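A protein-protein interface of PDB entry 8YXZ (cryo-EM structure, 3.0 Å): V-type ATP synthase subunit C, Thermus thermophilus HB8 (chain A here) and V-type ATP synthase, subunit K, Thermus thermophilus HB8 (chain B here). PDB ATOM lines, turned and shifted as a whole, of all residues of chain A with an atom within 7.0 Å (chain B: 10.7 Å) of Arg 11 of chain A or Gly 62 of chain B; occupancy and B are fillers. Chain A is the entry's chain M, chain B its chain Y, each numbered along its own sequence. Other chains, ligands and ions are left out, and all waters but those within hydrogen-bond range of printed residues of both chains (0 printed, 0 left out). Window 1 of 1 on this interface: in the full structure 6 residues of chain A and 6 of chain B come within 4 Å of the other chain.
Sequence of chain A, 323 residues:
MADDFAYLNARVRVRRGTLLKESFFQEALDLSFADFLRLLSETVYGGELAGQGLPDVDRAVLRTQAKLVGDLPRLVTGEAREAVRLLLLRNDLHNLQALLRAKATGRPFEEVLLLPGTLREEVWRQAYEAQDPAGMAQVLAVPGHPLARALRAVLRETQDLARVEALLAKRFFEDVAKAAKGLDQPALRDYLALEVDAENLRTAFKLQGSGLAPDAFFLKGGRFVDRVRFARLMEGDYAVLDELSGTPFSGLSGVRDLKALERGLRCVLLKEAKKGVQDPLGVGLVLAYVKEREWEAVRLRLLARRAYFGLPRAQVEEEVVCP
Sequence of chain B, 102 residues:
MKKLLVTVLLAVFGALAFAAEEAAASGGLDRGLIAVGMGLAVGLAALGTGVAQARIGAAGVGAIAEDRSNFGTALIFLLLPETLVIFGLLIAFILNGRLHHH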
ATOM      1  N   PHE A   5       9.211 -16.337  12.323  1.00  0.00           N
ATOM      2  CA  PHE A   5       8.084 -16.735  13.151  1.00  0.00           C
ATOM      3  C   PHE A   5       6.993 -17.490  12.388  1.00  0.00           C
ATOM      4  O   PHE A   5       6.288 -18.264  13.020  1.00  0.00           O
ATOM      5  CB  PHE A   5       7.515 -15.518  13.878  1.00  0.00           C
ATOM      6  CG  PHE A   5       8.357 -15.104  15.066  1.00  0.00           C
ATOM      7  CD1 PHE A   5       8.216 -15.786  16.283  1.00  0.00           C
ATOM      8  CD2 PHE A   5       9.306 -14.075  14.951  1.00  0.00           C
ATOM      9  CE1 PHE A   5       9.018 -15.444  17.382  1.00  0.00           C
ATOM     10  CE2 PHE A   5      10.092 -13.718  16.059  1.00  0.00           C
ATOM     11  CZ  PHE A   5       9.950 -14.406  17.271  1.00  0.00           C
ATOM     12  N   ALA A   6       6.885 -17.395  11.064  1.00  0.00           N
ATOM     13  CA  ALA A   6       6.008 -18.296  10.328  1.00  0.00           C
ATOM     14  C   ALA A   6       6.494 -19.748  10.440  1.00  0.00           C
ATOM     15  O   ALA A   6       5.689 -20.649  10.655  1.00  0.00           O
ATOM     16  CB  ALA A   6       5.911 -17.837   8.873  1.00  0.00           C
ATOM     17  N   TYR A   7       7.805 -19.986  10.370  1.00  0.00           N
ATOM     18  CA  TYR A   7       8.380 -21.315  10.568  1.00  0.00           C
ATOM     19  C   TYR A   7       8.233 -21.788  12.010  1.00  0.00           C
ATOM     20  O   TYR A   7       7.680 -22.856  12.257  1.00  0.00           O
ATOM     21  CB  TYR A   7       9.849 -21.286  10.174  1.00  0.00           C
ATOM     22  CG  TYR A   7      10.579 -22.583  10.404  1.00  0.00           C
ATOM     23  CD1 TYR A   7      10.362 -23.654   9.524  1.00  0.00           C
ATOM     24  CD2 TYR A   7      11.519 -22.706  11.444  1.00  0.00           C
ATOM     25  CE1 TYR A   7      11.143 -24.815   9.623  1.00  0.00           C
ATOM     26  CE2 TYR A   7      12.296 -23.873  11.555  1.00  0.00           C
ATOM     27  CZ  TYR A   7      12.137 -24.906  10.614  1.00  0.00           C
ATOM     28  OH  TYR A   7      12.974 -25.970  10.616  1.00  0.00           O
ATOM     29  N   LEU A   8       8.678 -20.991  12.980  1.00  0.00           N
ATOM     30  CA  LEU A   8       8.622 -21.394  14.381  1.00  0.00           C
ATOM     31  C   LEU A   8       7.188 -21.552  14.876  1.00  0.00           C
ATOM     32  O   LEU A   8       6.869 -22.569  15.482  1.00  0.00           O
ATOM     33  CB  LEU A   8       9.412 -20.409  15.244  1.00  0.00           C
ATOM     34  CG  LEU A   8       9.472 -20.811  16.725  1.00  0.00           C
ATOM     35  CD1 LEU A   8      10.203 -22.134  16.931  1.00  0.00           C
ATOM     36  CD2 LEU A   8      10.198 -19.743  17.531  1.00  0.00           C
ATOM     37  N   ASN A   9       6.289 -20.612  14.596  1.00  0.00           N
ATOM     38  CA  ASN A   9       4.926 -20.722  15.094  1.00  0.00           C
ATOM     39  C   ASN A   9       4.180 -21.885  14.445  1.00  0.00           C
ATOM     40  O   ASN A   9       3.312 -22.444  15.095  1.00  0.00           O
ATOM     41  CB  ASN A   9       4.160 -19.398  15.006  1.00  0.00           C
ATOM     42  CG  ASN A   9       4.734 -18.321  15.902  1.00  0.00           C
ATOM     43  OD1 ASN A   9       5.712 -18.508  16.599  1.00  0.00           O
ATOM     44  ND2 ASN A   9       4.115 -17.174  15.960  1.00  0.00           N
ATOM     45  N   ALA A  10       4.542 -22.342  13.247  1.00  0.00           N
ATOM     46  CA  ALA A  10       3.999 -23.591  12.732  1.00  0.00           C
ATOM     47  C   ALA A  10       4.408 -24.792  13.602  1.00  0.00           C
ATOM     48  O   ALA A  10       3.547 -25.572  13.999  1.00  0.00           O
ATOM     49  CB  ALA A  10       4.415 -23.764  11.274  1.00  0.00           C
ATOM     50  N   ARG A  11       5.685 -24.917  13.985  1.00  0.00           N
ATOM     51  CA  ARG A  11       6.130 -25.976  14.907  1.00  0.00           C
ATOM     52  C   ARG A  11       5.464 -25.865  16.273  1.00  0.00           C
ATOM     53  O   ARG A  11       4.979 -26.852  16.815  1.00  0.00           O
ATOM     54  CB  ARG A  11       7.639 -25.923  15.120  1.00  0.00           C
ATOM     55  CG  ARG A  11       8.469 -26.315  13.901  1.00  0.00           C
ATOM     56  CD  ARG A  11       9.918 -26.333  14.365  1.00  0.00           C
ATOM     57  NE  ARG A  11      10.839 -26.784  13.318  1.00  0.00           N
ATOM     58  CZ  ARG A  11      11.393 -27.975  13.251  1.00  0.00           C
ATOM     59  NH1 ARG A  11      12.399 -28.183  12.467  1.00  0.00           N
ATOM     60  NH2 ARG A  11      11.026 -28.997  13.950  1.00  0.00           N
ATOM     61  N   VAL A  12       5.406 -24.662  16.830  1.00  0.00           N
ATOM     62  CA  VAL A  12       4.782 -24.437  18.133  1.00  0.00           C
ATOM     63  C   VAL A  12       3.294 -24.746  18.088  1.00  0.00           C
ATOM     64  O   VAL A  12       2.812 -25.416  18.982  1.00  0.00           O
ATOM     65  CB  VAL A  12       5.065 -23.029  18.664  1.00  0.00           C
ATOM     66  CG1 VAL A  12       4.310 -22.740  19.956  1.00  0.00           C
ATOM     67  CG2 VAL A  12       6.555 -22.885  18.970  1.00  0.00           C
ATOM     68  N   ARG A  13       2.563 -24.375  17.032  1.00  0.00           N
ATOM     69  CA  ARG A  13       1.146 -24.730  16.860  1.00  0.00           C
ATOM     70  C   ARG A  13       0.941 -26.242  16.877  1.00  0.00           C
ATOM     71  O   ARG A  13       0.045 -26.705  17.569  1.00  0.00           O
ATOM     72  CB  ARG A  13       0.609 -24.119  15.562  1.00  0.00           C
ATOM     73  CG  ARG A  13       0.211 -22.640  15.691  1.00  0.00           C
ATOM     74  CD  ARG A  13      -1.134 -22.469  16.386  1.00  0.00           C
ATOM     75  NE  ARG A  13      -1.610 -21.081  16.352  1.00  0.00           N
ATOM     76  CZ  ARG A  13      -2.606 -20.576  17.051  1.00  0.00           C
ATOM     77  NH1 ARG A  13      -3.010 -19.370  16.823  1.00  0.00           N
ATOM     78  NH2 ARG A  13      -3.219 -21.236  17.981  1.00  0.00           N
ATOM     79  N   VAL A  14       1.797 -27.023  16.213  1.00  0.00           N
ATOM     80  CA  VAL A  14       1.736 -28.490  16.306  1.00  0.00           C
ATOM     81  C   VAL A  14       1.885 -28.948  17.753  1.00  0.00           C
ATOM     82  O   VAL A  14       1.011 -29.644  18.264  1.00  0.00           O
ATOM     83  CB  VAL A  14       2.785 -29.167  15.411  1.00  0.00           C
ATOM     84  CG1 VAL A  14       2.832 -30.680  15.615  1.00  0.00           C
ATOM     85  CG2 VAL A  14       2.495 -28.919  13.936  1.00  0.00           C
ATOM     86  N   ARG A  15       2.947 -28.532  18.453  1.00  0.00           N
ATOM     87  CA  ARG A  15       3.184 -28.949  19.846  1.00  0.00           C
ATOM     88  C   ARG A  15       2.071 -28.513  20.779  1.00  0.00           C
ATOM     89  O   ARG A  15       1.638 -29.286  21.621  1.00  0.00           O
ATOM     90  CB  ARG A  15       4.491 -28.366  20.377  1.00  0.00           C
ATOM     91  CG  ARG A  15       5.704 -28.972  19.691  1.00  0.00           C
ATOM     92  CD  ARG A  15       6.974 -28.404  20.305  1.00  0.00           C
ATOM     93  NE  ARG A  15       8.127 -28.911  19.574  1.00  0.00           N
ATOM     94  CZ  ARG A  15       9.393 -28.736  19.844  1.00  0.00           C
ATOM     95  NH1 ARG A  15      10.265 -29.204  19.020  1.00  0.00           N
ATOM     96  NH2 ARG A  15       9.803 -28.127  20.911  1.00  0.00           N
ATOM     97  N   ARG A  16       1.581 -27.289  20.621  1.00  0.00           N
ATOM     98  CA  ARG A  16       0.464 -26.727  21.386  1.00  0.00           C
ATOM     99  C   ARG A  16      -0.828 -27.515  21.199  1.00  0.00           C
ATOM    100  O   ARG A  16      -1.699 -27.463  22.055  1.00  0.00           O
ATOM    101  CB  ARG A  16       0.308 -25.258  20.983  1.00  0.00           C
ATOM    102  CG  ARG A  16      -0.646 -24.514  21.911  1.00  0.00           C
ATOM    103  CD  ARG A  16      -0.574 -23.007  21.691  1.00  0.00           C
ATOM    104  NE  ARG A  16      -1.437 -22.316  22.655  1.00  0.00           N
ATOM    105  CZ  ARG A  16      -2.747 -22.208  22.606  1.00  0.00           C
ATOM    106  NH1 ARG A  16      -3.390 -21.688  23.602  1.00  0.00           N
ATOM    107  NH2 ARG A  16      -3.446 -22.607  21.589  1.00  0.00           N
ATOM    108  N   GLY A  17      -0.948 -28.297  20.133  1.00  0.00           N
ATOM    109  CA  GLY A  17      -2.056 -29.223  19.950  1.00  0.00           C
ATOM    110  C   GLY A  17      -2.040 -30.377  20.952  1.00  0.00           C
ATOM    111  O   GLY A  17      -3.093 -30.791  21.425  1.00  0.00           O
ATOM    112  N   ASP A  71      14.513 -26.978  23.176  1.00  0.00           N
ATOM    113  CA  ASP A  71      15.063 -26.875  21.821  1.00  0.00           C
ATOM    114  C   ASP A  71      14.614 -25.613  21.068  1.00  0.00           C
ATOM    115  O   ASP A  71      15.216 -25.294  20.047  1.00  0.00           O
ATOM    116  CB  ASP A  71      14.730 -28.128  21.004  1.00  0.00           C
ATOM    117  CG  ASP A  71      13.235 -28.378  20.802  1.00  0.00           C
ATOM    118  OD1 ASP A  71      12.413 -27.765  21.511  1.00  0.00           O
ATOM    119  OD2 ASP A  71      12.873 -29.196  19.930  1.00  0.00           O
ATOM    120  N   LEU A  72      13.622 -24.858  21.545  1.00  0.00           N
ATOM    121  CA  LEU A  72      13.089 -23.703  20.821  1.00  0.00           C
ATOM    122  C   LEU A  72      14.166 -22.679  20.403  1.00  0.00           C
ATOM    123  O   LEU A  72      14.187 -22.319  19.227  1.00  0.00           O
ATOM    124  CB  LEU A  72      11.936 -23.059  21.609  1.00  0.00           C
ATOM    125  CG  LEU A  72      10.687 -23.941  21.731  1.00  0.00           C
ATOM    126  CD1 LEU A  72       9.751 -23.354  22.777  1.00  0.00           C
ATOM    127  CD2 LEU A  72       9.906 -24.021  20.430  1.00  0.00           C
ATOM    128  N   LEU A  75      16.097 -24.228  17.326  1.00  0.00           N
ATOM    129  CA  LEU A  75      15.358 -24.364  16.067  1.00  0.00           C
ATOM    130  C   LEU A  75      15.449 -23.104  15.198  1.00  0.00           C
ATOM    131  O   LEU A  75      15.591 -23.212  13.985  1.00  0.00           O
ATOM    132  CB  LEU A  75      13.892 -24.697  16.369  1.00  0.00           C
ATOM    133  CG  LEU A  75      13.690 -26.098  16.957  1.00  0.00           C
ATOM    134  CD1 LEU A  75      12.246 -26.236  17.423  1.00  0.00           C
ATOM    135  CD2 LEU A  75      13.983 -27.195  15.939  1.00  0.00           C
ATOM    136  N   TYR A 289       2.671 -20.573  24.885  1.00  0.00           N
ATOM    137  CA  TYR A 289       2.976 -21.995  24.858  1.00  0.00           C
ATOM    138  C   TYR A 289       3.952 -22.390  25.967  1.00  0.00           C
ATOM    139  O   TYR A 289       3.669 -23.303  26.738  1.00  0.00           O
ATOM    140  CB  TYR A 289       3.544 -22.374  23.498  1.00  0.00           C
ATOM    141  CG  TYR A 289       4.061 -23.788  23.478  1.00  0.00           C
ATOM    142  CD1 TYR A 289       3.145 -24.845  23.548  1.00  0.00           C
ATOM    143  CD2 TYR A 289       5.442 -24.044  23.456  1.00  0.00           C
ATOM    144  CE1 TYR A 289       3.603 -26.167  23.610  1.00  0.00           C
ATOM    145  CE2 TYR A 289       5.907 -25.367  23.532  1.00  0.00           C
ATOM    146  CZ  TYR A 289       4.983 -26.424  23.625  1.00  0.00           C
ATOM    147  OH  TYR A 289       5.420 -27.697  23.759  1.00  0.00           O
ATOM    148  N   ALA B  54       6.192 -17.372  -0.496  1.00  0.00           N
ATOM    149  CA  ALA B  54       7.292 -17.348   0.463  1.00  0.00           C
ATOM    150  C   ALA B  54       6.823 -17.719   1.866  1.00  0.00           C
ATOM    151  O   ALA B  54       7.221 -18.756   2.412  1.00  0.00           O
ATOM    152  CB  ALA B  54       7.954 -15.971   0.480  1.00  0.00           C
ATOM    153  N   ARG B  55       5.957 -16.887   2.447  1.00  0.00           N
ATOM    154  CA  ARG B  55       5.471 -17.158   3.795  1.00  0.00           C
ATOM    155  C   ARG B  55       4.645 -18.435   3.842  1.00  0.00           C
ATOM    156  O   ARG B  55       4.721 -19.194   4.820  1.00  0.00           O
ATOM    157  CB  ARG B  55       4.654 -15.977   4.313  1.00  0.00           C
ATOM    158  CG  ARG B  55       5.485 -14.792   4.754  1.00  0.00           C
ATOM    159  CD  ARG B  55       4.627 -13.772   5.474  1.00  0.00           C
ATOM    160  NE  ARG B  55       5.277 -12.471   5.557  1.00  0.00           N
ATOM    161  CZ  ARG B  55       5.856 -11.991   6.647  1.00  0.00           C
ATOM    162  NH1 ARG B  55       6.418 -10.787   6.607  1.00  0.00           N
ATOM    163  NH2 ARG B  55       5.886 -12.682   7.775  1.00  0.00           N
ATOM    164  N   ILE B  56       3.814 -18.747   2.853  1.00  0.00           N
ATOM    165  CA  ILE B  56       2.969 -19.949   2.982  1.00  0.00           C
ATOM    166  C   ILE B  56       3.819 -21.213   3.135  1.00  0.00           C
ATOM    167  O   ILE B  56       3.573 -22.028   4.021  1.00  0.00           O
ATOM    168  CB  ILE B  56       1.992 -20.096   1.809  1.00  0.00           C
ATOM    169  CG1 ILE B  56       1.037 -18.908   1.640  1.00  0.00           C
ATOM    170  CG2 ILE B  56       1.173 -21.377   1.998  1.00  0.00           C
ATOM    171  CD1 ILE B  56       0.250 -18.558   2.886  1.00  0.00           C
ATOM    172  N   GLY B  57       4.860 -21.362   2.324  1.00  0.00           N
ATOM    173  CA  GLY B  57       5.705 -22.545   2.395  1.00  0.00           C
ATOM    174  C   GLY B  57       6.680 -22.515   3.567  1.00  0.00           C
ATOM    175  O   GLY B  57       7.019 -23.575   4.074  1.00  0.00           O
ATOM    176  N   ALA B  58       7.072 -21.351   4.085  1.00  0.00           N
ATOM    177  CA  ALA B  58       7.868 -21.300   5.314  1.00  0.00           C
ATOM    178  C   ALA B  58       7.111 -21.880   6.515  1.00  0.00           C
ATOM    179  O   ALA B  58       7.671 -22.672   7.265  1.00  0.00           O
ATOM    180  CB  ALA B  58       8.308 -19.864   5.578  1.00  0.00           C
ATOM    181  N   ALA B  59       5.820 -21.569   6.663  1.00  0.00           N
ATOM    182  CA  ALA B  59       4.978 -22.212   7.663  1.00  0.00           C
ATOM    183  C   ALA B  59       4.801 -23.704   7.368  1.00  0.00           C
ATOM    184  O   ALA B  59       4.992 -24.538   8.245  1.00  0.00           O
ATOM    185  CB  ALA B  59       3.638 -21.483   7.725  1.00  0.00           C
ATOM    186  N   GLY B  60       4.504 -24.064   6.124  1.00  0.00           N
ATOM    187  CA  GLY B  60       4.306 -25.453   5.710  1.00  0.00           C
ATOM    188  C   GLY B  60       5.491 -26.367   6.018  1.00  0.00           C
ATOM    189  O   GLY B  60       5.305 -27.428   6.603  1.00  0.00           O
ATOM    190  N   VAL B  61       6.719 -25.949   5.719  1.00  0.00           N
ATOM    191  CA  VAL B  61       7.925 -26.728   6.045  1.00  0.00           C
ATOM    192  C   VAL B  61       8.090 -26.883   7.557  1.00  0.00           C
ATOM    193  O   VAL B  61       8.507 -27.938   8.018  1.00  0.00           O
ATOM    194  CB  VAL B  61       9.171 -26.100   5.398  1.00  0.00           C
ATOM    195  CG1 VAL B  61      10.474 -26.772   5.829  1.00  0.00           C
ATOM    196  CG2 VAL B  61       9.108 -26.225   3.875  1.00  0.00           C
ATOM    197  N   GLY B  62       7.694 -25.891   8.353  1.00  0.00           N
ATOM    198  CA  GLY B  62       7.704 -25.986   9.811  1.00  0.00           C
ATOM    199  C   GLY B  62       6.731 -27.036  10.335  1.00  0.00           C
ATOM    200  O   GLY B  62       7.111 -27.869  11.147  1.00  0.00           O
ATOM    201  N   ALA B  63       5.499 -27.070   9.831  1.00  0.00           N
ATOM    202  CA  ALA B  63       4.535 -28.095  10.218  1.00  0.00           C
ATOM    203  C   ALA B  63       4.953 -29.501   9.760  1.00  0.00           C
ATOM    204  O   ALA B  63       4.849 -30.449  10.526  1.00  0.00           O
ATOM    205  CB  ALA B  63       3.160 -27.715   9.677  1.00  0.00           C
ATOM    206  N   ILE B  64       5.460 -29.654   8.535  1.00  0.00           N
ATOM    207  CA  ILE B  64       5.946 -30.947   8.034  1.00  0.00           C
ATOM    208  C   ILE B  64       7.121 -31.446   8.866  1.00  0.00           C
ATOM    209  O   ILE B  64       7.198 -32.635   9.153  1.00  0.00           O
ATOM    210  CB  ILE B  64       6.348 -30.849   6.551  1.00  0.00           C
ATOM    211  CG1 ILE B  64       5.107 -30.721   5.656  1.00  0.00           C
ATOM    212  CG2 ILE B  64       7.159 -32.076   6.108  1.00  0.00           C
ATOM    213  CD1 ILE B  64       5.434 -30.159   4.267  1.00  0.00           C
ATOM    214  N   ALA B  65       8.038 -30.563   9.257  1.00  0.00           N
ATOM    215  CA  ALA B  65       9.181 -30.943  10.073  1.00  0.00           C
ATOM    216  C   ALA B  65       8.745 -31.461  11.444  1.00  0.00           C
ATOM    217  O   ALA B  65       9.279 -32.460  11.925  1.00  0.00           O
ATOM    218  CB  ALA B  65      10.118 -29.744  10.197  1.00  0.00           C
ATOM    219  N   GLU B  66       7.753 -30.825  12.062  1.00  0.00           N
ATOM    220  CA  GLU B  66       7.246 -31.261  13.359  1.00  0.00           C
ATOM    221  C   GLU B  66       6.407 -32.542  13.267  1.00  0.00           C
ATOM    222  O   GLU B  66       6.457 -33.364  14.177  1.00  0.00           O
ATOM    223  CB  GLU B  66       6.452 -30.123  14.010  1.00  0.00           C
ATOM    224  CG  GLU B  66       6.522 -30.161  15.540  1.00  0.00           C
ATOM    225  CD  GLU B  66       7.933 -29.934  16.105  1.00  0.00           C
ATOM    226  OE1 GLU B  66       8.770 -29.290  15.439  1.00  0.00           O
ATOM    227  OE2 GLU B  66       8.205 -30.389  17.238  1.00  0.00           O
ATOM    228  N   ASP B  67       5.665 -32.747  12.175  1.00  0.00           N
ATOM    229  CA  ASP B  67       4.909 -33.972  11.894  1.00  0.00           C
ATOM    230  C   ASP B  67       4.600 -34.120  10.392  1.00  0.00           C
ATOM    231  O   ASP B  67       3.836 -33.337   9.821  1.00  0.00           O
ATOM    232  CB  ASP B  67       3.618 -33.969  12.729  1.00  0.00           C
ATOM    233  CG  ASP B  67       2.666 -35.135  12.445  1.00  0.00           C
ATOM    234  OD1 ASP B  67       3.003 -36.051  11.665  1.00  0.00           O
ATOM    235  OD2 ASP B  67       1.572 -35.144  13.044  1.00  0.00           O
ATOM    236  N   ARG B  68       5.129 -35.177   9.758  1.00  0.00           N
ATOM    237  CA  ARG B  68       4.956 -35.451   8.325  1.00  0.00           C
ATOM    238  C   ARG B  68       3.509 -35.652   7.878  1.00  0.00           C
ATOM    239  O   ARG B  68       3.218 -35.468   6.704  1.00  0.00           O
ATOM    240  CB  ARG B  68       5.788 -36.669   7.921  1.00  0.00           C
ATOM    241  CG  ARG B  68       7.276 -36.340   7.809  1.00  0.00           C
ATOM    242  CD  ARG B  68       8.062 -37.595   7.409  1.00  0.00           C
ATOM    243  NE  ARG B  68       9.276 -37.280   6.637  1.00  0.00           N
ATOM    244  CZ  ARG B  68       9.336 -37.077   5.336  1.00  0.00           C
ATOM    245  NH1 ARG B  68      10.472 -37.004   4.719  1.00  0.00           N
ATOM    246  NH2 ARG B  68       8.258 -36.929   4.624  1.00  0.00           N
ATOM    247  N   SER B  69       2.579 -35.951   8.777  1.00  0.00           N
ATOM    248  CA  SER B  69       1.152 -36.034   8.436  1.00  0.00           C
ATOM    249  C   SER B  69       0.598 -34.719   7.864  1.00  0.00           C
ATOM    250  O   SER B  69      -0.335 -34.728   7.068  1.00  0.00           O
ATOM    251  CB  SER B  69       0.360 -36.451   9.677  1.00  0.00           C
ATOM    252  OG  SER B  69      -1.009 -36.623   9.368  1.00  0.00           O
ATOM    253  N   ASN B  70       1.199 -33.572   8.192  1.00  0.00           N
ATOM    254  CA  ASN B  70       0.784 -32.267   7.667  1.00  0.00           C
ATOM    255  C   ASN B  70       1.062 -32.045   6.167  1.00  0.00           C
ATOM    256  O   ASN B  70       0.686 -31.001   5.641  1.00  0.00           O
ATOM    257  CB  ASN B  70       1.443 -31.163   8.506  1.00  0.00           C
ATOM    258  CG  ASN B  70       0.960 -31.168   9.935  1.00  0.00           C
ATOM    259  OD1 ASN B  70      -0.182 -30.885  10.224  1.00  0.00           O
ATOM    260  ND2 ASN B  70       1.815 -31.488  10.869  1.00  0.00           N
ATOM    261  N   PHE B  71       1.724 -32.965   5.461  1.00  0.00           N
ATOM    262  CA  PHE B  71       2.201 -32.719   4.096  1.00  0.00           C
ATOM    263  C   PHE B  71       1.104 -32.281   3.115  1.00  0.00           C
ATOM    264  O   PHE B  71       1.282 -31.293   2.409  1.00  0.00           O
ATOM    265  CB  PHE B  71       2.950 -33.958   3.605  1.00  0.00           C
ATOM    266  CG  PHE B  71       3.570 -33.770   2.243  1.00  0.00           C
ATOM    267  CD1 PHE B  71       4.853 -33.214   2.124  1.00  0.00           C
ATOM    268  CD2 PHE B  71       2.851 -34.115   1.088  1.00  0.00           C
ATOM    269  CE1 PHE B  71       5.408 -32.989   0.853  1.00  0.00           C
ATOM    270  CE2 PHE B  71       3.409 -33.894  -0.181  1.00  0.00           C
ATOM    271  CZ  PHE B  71       4.685 -33.323  -0.300  1.00  0.00           C
ATOM    272  N   THR B  73      -1.952 -30.809   3.705  1.00  0.00           N
ATOM    273  CA  THR B  73      -2.351 -29.460   4.113  1.00  0.00           C
ATOM    274  C   THR B  73      -1.354 -28.409   3.652  1.00  0.00           C
ATOM    275  O   THR B  73      -1.739 -27.422   3.033  1.00  0.00           O
ATOM    276  CB  THR B  73      -2.464 -29.388   5.634  1.00  0.00           C
ATOM    277  OG1 THR B  73      -3.303 -30.412   6.108  1.00  0.00           O
ATOM    278  CG2 THR B  73      -2.980 -28.046   6.130  1.00  0.00           C
ATOM    279  N   ALA B  74      -0.066 -28.622   3.911  1.00  0.00           N
ATOM    280  CA  ALA B  74       0.971 -27.679   3.520  1.00  0.00           C
ATOM    281  C   ALA B  74       1.031 -27.489   1.998  1.00  0.00           C
ATOM    282  O   ALA B  74       1.121 -26.359   1.524  1.00  0.00           O
ATOM    283  CB  ALA B  74       2.295 -28.191   4.083  1.00  0.00           C
ATOM    284  N   LEU B  75       0.933 -28.576   1.231  1.00  0.00           N
ATOM    285  CA  LEU B  75       0.961 -28.535  -0.226  1.00  0.00           C
ATOM    286  C   LEU B  75      -0.278 -27.849  -0.816  1.00  0.00           C
ATOM    287  O   LEU B  75      -0.147 -27.029  -1.713  1.00  0.00           O
ATOM    288  CB  LEU B  75       1.132 -29.966  -0.748  1.00  0.00           C
ATOM    289  CG  LEU B  75       1.400 -30.058  -2.253  1.00  0.00           C
ATOM    290  CD1 LEU B  75       2.729 -29.426  -2.636  1.00  0.00           C
ATOM    291  CD2 LEU B  75       1.447 -31.517  -2.673  1.00  0.00           C
ATOM    292  N   LEU B  78       0.199 -24.067  -0.247  1.00  0.00           N
ATOM    293  CA  LEU B  78       1.258 -23.542  -1.110  1.00  0.00           C
ATOM    294  C   LEU B  78       0.827 -23.353  -2.573  1.00  0.00           C
ATOM    295  O   LEU B  78       1.308 -22.437  -3.234  1.00  0.00           O
ATOM    296  CB  LEU B  78       2.479 -24.467  -1.003  1.00  0.00           C
ATOM    297  CG  LEU B  78       3.690 -24.035  -1.841  1.00  0.00           C
ATOM    298  CD1 LEU B  78       4.248 -22.692  -1.376  1.00  0.00           C
ATOM    299  CD2 LEU B  78       4.793 -25.066  -1.716  1.00  0.00           C
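The guanidinium group (NE) of Arg 15 of chain A is in salt-bridge range of the side-chain carboxylate (OE2) of Glu 66 of chain B. The guanidinium group (NH2) of Arg 11 of chain A lies within salt-bridge range of the side-chain carboxylate (OE1) of Glu 66 of chain B (2.7 Å).
NH2 of Arg 15 of chain A is in salt-bridge range of OD1 of Asp 71 of chain A (2.7 Å). NH1 of Arg 11 of chain A lies within hydrogen-bond range of OH of Tyr 7 of chain A, at 2.9 Å. ND2 of Asn 70 of chain B sits at hydrogen-bond distance from O of Ala 63 of chain B, 3.2 Å away.
Among the printed residues, pairs that only touch across the chains: Ala 10 of chain A with Ala 59 of chain B, Arg 11 of chain A with Gly 62 of chain B, Ala 6 of chain A with Ala 59 of chain B, Tyr 7 of chain A with Gly 62 of chain B, Arg 11 of chain A with Ala 65 of chain B, Tyr 7 of chain A with Ala 58 of chain B, Val 14 of chain A with Glu 66 of chain B and Ala 10 of chain A with Ala 63 of chain B.
Of the printed residues of chain B, Ala 6 of chain A touches Ala 59. Of the printed residues of chain B, Tyr 7 of chain A touches Ala 58 and Gly 62. Of chain B, only Ala 59 and Ala 63 come within 4 Å of Ala 10 of chain A. No residue of chain B comes within 4 Å of Val 12 of chain A. Of chain B, only Glu 66 comes within 4 Å of Val 14 of chain A. Val 61 of chain B touches none of the printed residues of chain A. Of chain A, only Tyr 7 and Arg 11 come within 4 Å of Gly 62 of chain B. Printed residues of chain A within 4 Å of Ala 65 of chain B: Arg 11. The nearest residue of chain A that does not touch Gly 62 of chain B is Ala 10 of chain A (4.1 Å). The nearest printed residue of chain A that does not touch Ala 58 of chain B is Ala 6 of chain A (4.4 Å).
Hydrophobic or aromatic side chains of chain A that line the printed part of chain B: Tyr 7, Ala 10 and Val 14. Among the printed residues, Asp or Glu carboxylates within 4 Å of a Lys or Arg side-chain nitrogen of the other chain: Arg 11 of chain A with Glu 66 of chain B and Arg 15 of chain A with Glu 66 of chain B.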
